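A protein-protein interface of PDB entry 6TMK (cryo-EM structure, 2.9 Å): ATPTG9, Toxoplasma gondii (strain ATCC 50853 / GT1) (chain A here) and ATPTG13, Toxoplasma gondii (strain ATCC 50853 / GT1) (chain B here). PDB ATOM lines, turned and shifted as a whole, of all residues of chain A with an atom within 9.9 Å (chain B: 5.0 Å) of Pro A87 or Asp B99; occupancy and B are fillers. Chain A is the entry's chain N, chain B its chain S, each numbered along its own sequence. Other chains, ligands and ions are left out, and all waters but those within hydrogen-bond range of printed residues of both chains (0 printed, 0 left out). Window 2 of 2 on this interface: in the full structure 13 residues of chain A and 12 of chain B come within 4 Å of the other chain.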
ATOM      1  N   LYS A  22       6.870  23.598  28.825  1.00  0.00           N
ATOM      2  CA  LYS A  22       5.638  23.083  28.237  1.00  0.00           C
ATOM      3  C   LYS A  22       4.498  23.103  29.245  1.00  0.00           C
ATOM      4  O   LYS A  22       3.362  23.451  28.902  1.00  0.00           O
ATOM      5  CB  LYS A  22       5.857  21.667  27.714  1.00  0.00           C
ATOM      6  CG  LYS A  22       6.779  21.580  26.523  1.00  0.00           C
ATOM      7  CD  LYS A  22       7.045  20.138  26.150  1.00  0.00           C
ATOM      8  CE  LYS A  22       7.197  19.968  24.657  1.00  0.00           C
ATOM      9  NZ  LYS A  22       7.602  18.584  24.312  1.00  0.00           N
ATOM     10  N   GLY A  51      23.267  21.345  20.432  1.00  0.00           N
ATOM     11  CA  GLY A  51      22.874  21.139  19.054  1.00  0.00           C
ATOM     12  C   GLY A  51      21.411  20.815  18.879  1.00  0.00           C
ATOM     13  O   GLY A  51      21.020  20.283  17.838  1.00  0.00           O
ATOM     14  N   THR A  52      20.589  21.120  19.876  1.00  0.00           N
ATOM     15  CA  THR A  52      19.181  20.763  19.897  1.00  0.00           C
ATOM     16  C   THR A  52      18.334  21.928  19.394  1.00  0.00           C
ATOM     17  O   THR A  52      18.762  23.085  19.397  1.00  0.00           O
ATOM     18  CB  THR A  52      18.754  20.369  21.315  1.00  0.00           C
ATOM     19  OG1 THR A  52      19.581  19.297  21.783  1.00  0.00           O
ATOM     20  CG2 THR A  52      17.307  19.921  21.338  1.00  0.00           C
ATOM     21  N   SER A  53      17.127  21.603  18.939  1.00  0.00           N
ATOM     22  CA  SER A  53      16.108  22.592  18.624  1.00  0.00           C
ATOM     23  C   SER A  53      14.838  22.314  19.419  1.00  0.00           C
ATOM     24  O   SER A  53      14.504  21.161  19.706  1.00  0.00           O
ATOM     25  CB  SER A  53      15.795  22.598  17.128  1.00  0.00           C
ATOM     26  OG  SER A  53      16.942  22.956  16.378  1.00  0.00           O
ATOM     27  N   TYR A  54      14.131  23.391  19.773  1.00  0.00           N
ATOM     28  CA  TYR A  54      12.960  23.311  20.635  1.00  0.00           C
ATOM     29  C   TYR A  54      11.749  24.031  20.049  1.00  0.00           C
ATOM     30  O   TYR A  54      10.742  24.196  20.748  1.00  0.00           O
ATOM     31  CB  TYR A  54      13.281  23.876  22.023  1.00  0.00           C
ATOM     32  CG  TYR A  54      14.161  22.977  22.856  1.00  0.00           C
ATOM     33  CD1 TYR A  54      13.707  21.744  23.295  1.00  0.00           C
ATOM     34  CD2 TYR A  54      15.445  23.361  23.205  1.00  0.00           C
ATOM     35  CE1 TYR A  54      14.506  20.919  24.053  1.00  0.00           C
ATOM     36  CE2 TYR A  54      16.251  22.541  23.964  1.00  0.00           C
ATOM     37  CZ  TYR A  54      15.778  21.323  24.385  1.00  0.00           C
ATOM     38  OH  TYR A  54      16.580  20.504  25.144  1.00  0.00           O
ATOM     39  N   CYS A  55      11.819  24.463  18.790  1.00  0.00           N
ATOM     40  CA  CYS A  55      10.665  24.978  18.052  1.00  0.00           C
ATOM     41  C   CYS A  55      10.059  26.208  18.726  1.00  0.00           C
ATOM     42  O   CYS A  55       8.848  26.442  18.650  1.00  0.00           O
ATOM     43  CB  CYS A  55       9.598  23.892  17.893  1.00  0.00           C
ATOM     44  SG  CYS A  55      10.095  22.454  16.907  1.00  0.00           S
ATOM     45  N   PHE A  78       1.709  26.423  10.507  1.00  0.00           N
ATOM     46  CA  PHE A  78       1.363  25.083  10.967  1.00  0.00           C
ATOM     47  C   PHE A  78       2.360  24.054  10.453  1.00  0.00           C
ATOM     48  O   PHE A  78       2.886  23.240  11.223  1.00  0.00           O
ATOM     49  CB  PHE A  78      -0.045  24.732  10.503  1.00  0.00           C
ATOM     50  CG  PHE A  78      -1.121  25.202  11.419  1.00  0.00           C
ATOM     51  CD1 PHE A  78      -1.293  24.628  12.655  1.00  0.00           C
ATOM     52  CD2 PHE A  78      -1.968  26.217  11.041  1.00  0.00           C
ATOM     53  CE1 PHE A  78      -2.281  25.056  13.490  1.00  0.00           C
ATOM     54  CE2 PHE A  78      -2.958  26.648  11.878  1.00  0.00           C
ATOM     55  CZ  PHE A  78      -3.112  26.069  13.103  1.00  0.00           C
ATOM     56  N   VAL A  79       2.620  24.068   9.146  1.00  0.00           N
ATOM     57  CA  VAL A  79       3.530  23.079   8.584  1.00  0.00           C
ATOM     58  C   VAL A  79       4.952  23.304   9.081  1.00  0.00           C
ATOM     59  O   VAL A  79       5.700  22.341   9.285  1.00  0.00           O
ATOM     60  CB  VAL A  79       3.447  23.101   7.047  1.00  0.00           C
ATOM     61  CG1 VAL A  79       3.996  24.376   6.509  1.00  0.00           C
ATOM     62  CG2 VAL A  79       4.207  21.943   6.459  1.00  0.00           C
ATOM     63  N   ALA A  80       5.346  24.558   9.312  1.00  0.00           N
ATOM     64  CA  ALA A  80       6.672  24.824   9.851  1.00  0.00           C
ATOM     65  C   ALA A  80       6.833  24.228  11.239  1.00  0.00           C
ATOM     66  O   ALA A  80       7.859  23.613  11.544  1.00  0.00           O
ATOM     67  CB  ALA A  80       6.923  26.325   9.890  1.00  0.00           C
ATOM     68  N   MET A  81       5.829  24.406  12.096  1.00  0.00           N
ATOM     69  CA  MET A  81       5.884  23.820  13.429  1.00  0.00           C
ATOM     70  C   MET A  81       5.914  22.300  13.354  1.00  0.00           C
ATOM     71  O   MET A  81       6.690  21.644  14.065  1.00  0.00           O
ATOM     72  CB  MET A  81       4.692  24.298  14.253  1.00  0.00           C
ATOM     73  CG  MET A  81       4.727  23.876  15.704  1.00  0.00           C
ATOM     74  SD  MET A  81       6.148  24.530  16.589  1.00  0.00           S
ATOM     75  CE  MET A  81       6.226  23.389  17.964  1.00  0.00           C
ATOM     76  N   ARG A  82       5.074  21.727  12.493  1.00  0.00           N
ATOM     77  CA  ARG A  82       5.028  20.278  12.357  1.00  0.00           C
ATOM     78  C   ARG A  82       6.371  19.721  11.915  1.00  0.00           C
ATOM     79  O   ARG A  82       6.785  18.649  12.369  1.00  0.00           O
ATOM     80  CB  ARG A  82       3.941  19.891  11.359  1.00  0.00           C
ATOM     81  CG  ARG A  82       3.715  18.411  11.239  1.00  0.00           C
ATOM     82  CD  ARG A  82       4.394  17.828  10.026  1.00  0.00           C
ATOM     83  NE  ARG A  82       4.088  16.415   9.873  1.00  0.00           N
ATOM     84  CZ  ARG A  82       4.567  15.464  10.663  1.00  0.00           C
ATOM     85  NH1 ARG A  82       5.374  15.765  11.667  1.00  0.00           N
ATOM     86  NH2 ARG A  82       4.230  14.207  10.451  1.00  0.00           N
ATOM     87  N   GLU A  83       7.063  20.425  11.022  1.00  0.00           N
ATOM     88  CA  GLU A  83       8.332  19.922  10.518  1.00  0.00           C
ATOM     89  C   GLU A  83       9.491  20.216  11.458  1.00  0.00           C
ATOM     90  O   GLU A  83      10.473  19.469  11.471  1.00  0.00           O
ATOM     91  CB  GLU A  83       8.623  20.522   9.147  1.00  0.00           C
ATOM     92  CG  GLU A  83       7.631  20.120   8.086  1.00  0.00           C
ATOM     93  CD  GLU A  83       7.741  18.658   7.710  1.00  0.00           C
ATOM     94  OE1 GLU A  83       8.801  18.052   7.970  1.00  0.00           O
ATOM     95  OE2 GLU A  83       6.764  18.108   7.164  1.00  0.00           O
ATOM     96  N   CYS A  84       9.400  21.284  12.249  1.00  0.00           N
ATOM     97  CA  CYS A  84      10.408  21.528  13.272  1.00  0.00           C
ATOM     98  C   CYS A  84      10.343  20.474  14.365  1.00  0.00           C
ATOM     99  O   CYS A  84      11.381  19.985  14.825  1.00  0.00           O
ATOM    100  CB  CYS A  84      10.238  22.925  13.867  1.00  0.00           C
ATOM    101  SG  CYS A  84      11.204  23.198  15.377  1.00  0.00           S
ATOM    102  N   ASN A  85       9.136  20.109  14.798  1.00  0.00           N
ATOM    103  CA  ASN A  85       9.015  19.217  15.945  1.00  0.00           C
ATOM    104  C   ASN A  85       9.458  17.792  15.650  1.00  0.00           C
ATOM    105  O   ASN A  85       9.426  16.960  16.563  1.00  0.00           O
ATOM    106  CB  ASN A  85       7.572  19.204  16.446  1.00  0.00           C
ATOM    107  CG  ASN A  85       7.474  18.941  17.931  1.00  0.00           C
ATOM    108  OD1 ASN A  85       7.868  19.770  18.747  1.00  0.00           O
ATOM    109  ND2 ASN A  85       6.951  17.775  18.290  1.00  0.00           N
ATOM    110  N   ARG A  86       9.862  17.482  14.425  1.00  0.00           N
ATOM    111  CA  ARG A  86      10.367  16.154  14.131  1.00  0.00           C
ATOM    112  C   ARG A  86      11.727  15.940  14.797  1.00  0.00           C
ATOM    113  O   ARG A  86      12.514  16.881  14.933  1.00  0.00           O
ATOM    114  CB  ARG A  86      10.484  15.964  12.630  1.00  0.00           C
ATOM    115  CG  ARG A  86       9.236  15.424  12.004  1.00  0.00           C
ATOM    116  CD  ARG A  86       9.366  15.322  10.511  1.00  0.00           C
ATOM    117  NE  ARG A  86       8.429  14.351   9.955  1.00  0.00           N
ATOM    118  CZ  ARG A  86       7.669  14.557   8.886  1.00  0.00           C
ATOM    119  NH1 ARG A  86       7.722  15.700   8.223  1.00  0.00           N
ATOM    120  NH2 ARG A  86       6.852  13.607   8.470  1.00  0.00           N
ATOM    121  N   PRO A  87      12.040  14.702  15.211  1.00  0.00           N
ATOM    122  CA  PRO A  87      13.298  14.473  15.936  1.00  0.00           C
ATOM    123  C   PRO A  87      14.542  14.678  15.087  1.00  0.00           C
ATOM    124  O   PRO A  87      15.452  15.418  15.470  1.00  0.00           O
ATOM    125  CB  PRO A  87      13.184  13.009  16.382  1.00  0.00           C
ATOM    126  CG  PRO A  87      11.758  12.644  16.193  1.00  0.00           C
ATOM    127  CD  PRO A  87      11.289  13.452  15.047  1.00  0.00           C
ATOM    128  N   GLN A  88      14.588  14.023  13.931  1.00  0.00           N
ATOM    129  CA  GLN A  88      15.769  14.049  13.080  1.00  0.00           C
ATOM    130  C   GLN A  88      15.843  15.291  12.208  1.00  0.00           C
ATOM    131  O   GLN A  88      16.832  15.463  11.486  1.00  0.00           O
ATOM    132  CB  GLN A  88      15.813  12.799  12.202  1.00  0.00           C
ATOM    133  CG  GLN A  88      15.994  11.514  12.975  1.00  0.00           C
ATOM    134  CD  GLN A  88      16.315  10.340  12.079  1.00  0.00           C
ATOM    135  OE1 GLN A  88      16.094  10.388  10.871  1.00  0.00           O
ATOM    136  NE2 GLN A  88      16.849   9.279  12.666  1.00  0.00           N
ATOM    137  N   GLY A  89      14.832  16.148  12.251  1.00  0.00           N
ATOM    138  CA  GLY A  89      14.829  17.364  11.480  1.00  0.00           C
ATOM    139  C   GLY A  89      13.702  17.406  10.472  1.00  0.00           C
ATOM    140  O   GLY A  89      12.982  16.425  10.259  1.00  0.00           O
ATOM    141  N   PRO A  90      13.532  18.555   9.826  1.00  0.00           N
ATOM    142  CA  PRO A  90      12.421  18.722   8.883  1.00  0.00           C
ATOM    143  C   PRO A  90      12.662  17.954   7.593  1.00  0.00           C
ATOM    144  O   PRO A  90      13.747  18.006   7.012  1.00  0.00           O
ATOM    145  CB  PRO A  90      12.391  20.233   8.644  1.00  0.00           C
ATOM    146  CG  PRO A  90      13.785  20.664   8.870  1.00  0.00           C
ATOM    147  CD  PRO A  90      14.316  19.791   9.970  1.00  0.00           C
ATOM    148  N   HIS A  91      11.633  17.228   7.154  1.00  0.00           N
ATOM    149  CA  HIS A  91      11.673  16.585   5.849  1.00  0.00           C
ATOM    150  C   HIS A  91      11.299  17.564   4.747  1.00  0.00           C
ATOM    151  O   HIS A  91      11.919  17.574   3.679  1.00  0.00           O
ATOM    152  CB  HIS A  91      10.717  15.395   5.821  1.00  0.00           C
ATOM    153  CG  HIS A  91      11.046  14.325   6.810  1.00  0.00           C
ATOM    154  ND1 HIS A  91      10.280  13.189   6.954  1.00  0.00           N
ATOM    155  CD2 HIS A  91      12.054  14.214   7.705  1.00  0.00           C
ATOM    156  CE1 HIS A  91      10.802  12.427   7.897  1.00  0.00           C
ATOM    157  NE2 HIS A  91      11.879  13.025   8.368  1.00  0.00           N
ATOM    158  N   TYR A 114       9.564   9.284  -0.020  1.00  0.00           N
ATOM    159  CA  TYR A 114       8.494   9.956  -0.732  1.00  0.00           C
ATOM    160  C   TYR A 114       8.506   9.536  -2.193  1.00  0.00           C
ATOM    161  O   TYR A 114       9.554   9.213  -2.758  1.00  0.00           O
ATOM    162  CB  TYR A 114       8.631  11.470  -0.615  1.00  0.00           C
ATOM    163  CG  TYR A 114       8.444  11.969   0.793  1.00  0.00           C
ATOM    164  CD1 TYR A 114       7.185  12.250   1.287  1.00  0.00           C
ATOM    165  CD2 TYR A 114       9.528  12.146   1.634  1.00  0.00           C
ATOM    166  CE1 TYR A 114       7.011  12.697   2.567  1.00  0.00           C
ATOM    167  CE2 TYR A 114       9.362  12.592   2.917  1.00  0.00           C
ATOM    168  CZ  TYR A 114       8.100  12.867   3.382  1.00  0.00           C
ATOM    169  OH  TYR A 114       7.922  13.316   4.670  1.00  0.00           O
ATOM    170  N   ARG B  95       0.045  14.994  14.973  1.00  0.00           N
ATOM    171  CA  ARG B  95       1.383  14.866  14.409  1.00  0.00           C
ATOM    172  C   ARG B  95       2.454  14.985  15.487  1.00  0.00           C
ATOM    173  O   ARG B  95       3.480  14.298  15.432  1.00  0.00           O
ATOM    174  CB  ARG B  95       1.586  15.923  13.330  1.00  0.00           C
ATOM    175  CG  ARG B  95       0.598  15.840  12.197  1.00  0.00           C
ATOM    176  CD  ARG B  95       0.804  14.628  11.319  1.00  0.00           C
ATOM    177  NE  ARG B  95       0.194  13.413  11.848  1.00  0.00           N
ATOM    178  CZ  ARG B  95      -1.114  13.214  11.952  1.00  0.00           C
ATOM    179  NH1 ARG B  95      -1.574  12.075  12.437  1.00  0.00           N
ATOM    180  NH2 ARG B  95      -1.962  14.152  11.578  1.00  0.00           N
ATOM    181  N   MET B  96       2.230  15.840  16.482  1.00  0.00           N
ATOM    182  CA  MET B  96       3.185  15.971  17.575  1.00  0.00           C
ATOM    183  C   MET B  96       3.241  14.699  18.412  1.00  0.00           C
ATOM    184  O   MET B  96       4.318  14.287  18.862  1.00  0.00           O
ATOM    185  CB  MET B  96       2.820  17.175  18.432  1.00  0.00           C
ATOM    186  CG  MET B  96       3.087  18.498  17.749  1.00  0.00           C
ATOM    187  SD  MET B  96       2.357  19.905  18.587  1.00  0.00           S
ATOM    188  CE  MET B  96       3.619  20.231  19.801  1.00  0.00           C
ATOM    189  N   LEU B  97       2.093  14.057  18.622  1.00  0.00           N
ATOM    190  CA  LEU B  97       2.102  12.769  19.311  1.00  0.00           C
ATOM    191  C   LEU B  97       2.891  11.730  18.524  1.00  0.00           C
ATOM    192  O   LEU B  97       3.674  10.957  19.097  1.00  0.00           O
ATOM    193  CB  LEU B  97       0.677  12.286  19.542  1.00  0.00           C
ATOM    194  CG  LEU B  97      -0.182  13.132  20.475  1.00  0.00           C
ATOM    195  CD1 LEU B  97      -1.573  12.574  20.546  1.00  0.00           C
ATOM    196  CD2 LEU B  97       0.421  13.213  21.844  1.00  0.00           C
ATOM    197  N   GLU B  98       2.692  11.692  17.206  1.00  0.00           N
ATOM    198  CA  GLU B  98       3.474  10.788  16.368  1.00  0.00           C
ATOM    199  C   GLU B  98       4.966  11.068  16.494  1.00  0.00           C
ATOM    200  O   GLU B  98       5.781  10.139  16.532  1.00  0.00           O
ATOM    201  CB  GLU B  98       3.038  10.929  14.916  1.00  0.00           C
ATOM    202  CG  GLU B  98       1.731  10.271  14.586  1.00  0.00           C
ATOM    203  CD  GLU B  98       1.292  10.560  13.167  1.00  0.00           C
ATOM    204  OE1 GLU B  98       2.071  11.186  12.420  1.00  0.00           O
ATOM    205  OE2 GLU B  98       0.164  10.171  12.799  1.00  0.00           O
ATOM    206  N   ASP B  99       5.342  12.345  16.547  1.00  0.00           N
ATOM    207  CA  ASP B  99       6.751  12.695  16.669  1.00  0.00           C
ATOM    208  C   ASP B  99       7.321  12.227  18.001  1.00  0.00           C
ATOM    209  O   ASP B  99       8.463  11.762  18.065  1.00  0.00           O
ATOM    210  CB  ASP B  99       6.933  14.200  16.507  1.00  0.00           C
ATOM    211  CG  ASP B  99       6.606  14.678  15.107  1.00  0.00           C
ATOM    212  OD1 ASP B  99       6.585  13.840  14.181  1.00  0.00           O
ATOM    213  OD2 ASP B  99       6.371  15.893  14.931  1.00  0.00           O
ATOM    214  N   GLU B 100       6.542  12.345  19.074  1.00  0.00           N
ATOM    215  CA  GLU B 100       6.989  11.837  20.368  1.00  0.00           C
ATOM    216  C   GLU B 100       7.216  10.332  20.311  1.00  0.00           C
ATOM    217  O   GLU B 100       8.227   9.815  20.813  1.00  0.00           O
ATOM    218  CB  GLU B 100       5.965  12.181  21.444  1.00  0.00           C
ATOM    219  CG  GLU B 100       6.378  11.769  22.835  1.00  0.00           C
ATOM    220  CD  GLU B 100       5.390  12.224  23.890  1.00  0.00           C
ATOM    221  OE1 GLU B 100       5.480  11.745  25.042  1.00  0.00           O
ATOM    222  OE2 GLU B 100       4.522  13.063  23.569  1.00  0.00           O
ATOM    223  N   VAL B 101       6.275   9.610  19.707  1.00  0.00           N
ATOM    224  CA  VAL B 101       6.421   8.163  19.584  1.00  0.00           C
ATOM    225  C   VAL B 101       7.683   7.819  18.805  1.00  0.00           C
ATOM    226  O   VAL B 101       8.434   6.912  19.182  1.00  0.00           O
ATOM    227  CB  VAL B 101       5.169   7.558  18.926  1.00  0.00           C
ATOM    228  CG1 VAL B 101       5.406   6.108  18.570  1.00  0.00           C
ATOM    229  CG2 VAL B 101       3.986   7.689  19.845  1.00  0.00           C
ATOM    230  N   GLU B 102       7.930   8.522  17.700  1.00  0.00           N
ATOM    231  CA  GLU B 102       9.130   8.261  16.914  1.00  0.00           C
ATOM    232  C   GLU B 102      10.395   8.556  17.711  1.00  0.00           C
ATOM    233  O   GLU B 102      11.388   7.826  17.610  1.00  0.00           O
ATOM    234  CB  GLU B 102       9.103   9.089  15.634  1.00  0.00           C
ATOM    235  CG  GLU B 102      10.231   8.776  14.673  1.00  0.00           C
ATOM    236  CD  GLU B 102       9.994   9.330  13.284  1.00  0.00           C
ATOM    237  OE1 GLU B 102      10.944   9.894  12.701  1.00  0.00           O
ATOM    238  OE2 GLU B 102       8.862   9.199  12.772  1.00  0.00           O
ATOM    239  N   ARG B 103      10.385   9.637  18.492  1.00  0.00           N
ATOM    240  CA  ARG B 103      11.549   9.966  19.304  1.00  0.00           C
ATOM    241  C   ARG B 103      11.838   8.870  20.314  1.00  0.00           C
ATOM    242  O   ARG B 103      13.002   8.572  20.602  1.00  0.00           O
ATOM    243  CB  ARG B 103      11.345  11.299  20.015  1.00  0.00           C
ATOM    244  CG  ARG B 103      12.600  11.806  20.698  1.00  0.00           C
ATOM    245  CD  ARG B 103      12.467  13.221  21.236  1.00  0.00           C
ATOM    246  NE  ARG B 103      12.069  14.179  20.208  1.00  0.00           N
ATOM    247  CZ  ARG B 103      10.834  14.644  20.038  1.00  0.00           C
ATOM    248  NH1 ARG B 103       9.843  14.251  20.825  1.00  0.00           N
ATOM    249  NH2 ARG B 103      10.589  15.509  19.067  1.00  0.00           N
ATOM    250  N   LEU B 106      13.316   5.705  18.308  1.00  0.00           N
ATOM    251  CA  LEU B 106      14.692   5.811  17.838  1.00  0.00           C
ATOM    252  C   LEU B 106      15.709   5.465  18.916  1.00  0.00           C
ATOM    253  O   LEU B 106      16.882   5.249  18.597  1.00  0.00           O
ATOM    254  CB  LEU B 106      14.961   7.218  17.318  1.00  0.00           C
ATOM    255  CG  LEU B 106      14.207   7.622  16.051  1.00  0.00           C
ATOM    256  CD1 LEU B 106      14.521   9.057  15.702  1.00  0.00           C
ATOM    257  CD2 LEU B 106      14.528   6.708  14.894  1.00  0.00           C
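The backbone NH (N) of Asn A85 lies within hydrogen-bond range of the side-chain sulfur (SG) of Cys A55 (3.3 Å). NH1 of Arg B95 is in salt-bridge range of OE2 of Glu B98 (2.6 Å). The side-chain sulfur (SG) of Cys A55 forms a disulfide with the side-chain sulfur (SG) of Cys A84. OE1 of Glu A83 lies within salt-bridge range of NH1 of Arg A86 (2.6 Å).
O of Asn A85 sits at hydrogen-bond distance from NH2 of Arg B103 (3.1 Å). The guanidinium group (NH1) of Arg A82 lies within salt-bridge range of the side-chain carboxylate (OD1) of Asp B99.
Among the printed residues, pairs that only touch across the chains: Arg A82 with Arg B95 (3.6 Å), Asn A85 with Met B96 (3.97 Å), Asn A85 with Asp B99 (3.6 Å), Arg A86 with Asp B99 (3.8 Å), Pro A87 with Asp B99 (3.9 Å) and Gln A88 with Leu B106 (3.8 Å).
Hydrophobic or aromatic side chains of chain A within 4 Å of the printed part of chain B: Pro A87. Along chain A the printed residues that touch a printed residue of chain B span positions 82 to 88. Hydrophobic or aromatic side chains of chain B within 4 Å of the printed part of chain A: Met B96 and Leu B106. Among the printed residues, 8 pairs touch across the chains.
Of chain B, only Asp B99 comes within 4 Å of Pro A87. No residue of chain A comes within 4 Å of Glu B102. Printed residues of chain B within 4 Å of Gln A88: Leu B106. Of the printed residues of chain B, Asn A85 touches Met B96, Asp B99 and Arg B103. Of the printed residues of chain B, Arg A82 touches Arg B95 and Asp B99. Printed residues of chain A within 4 Å of Leu B106: Gln A88 (3.8 Å). The nearest residue of chain A that does not touch Asp B99 is Met A81 (5.8 Å).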
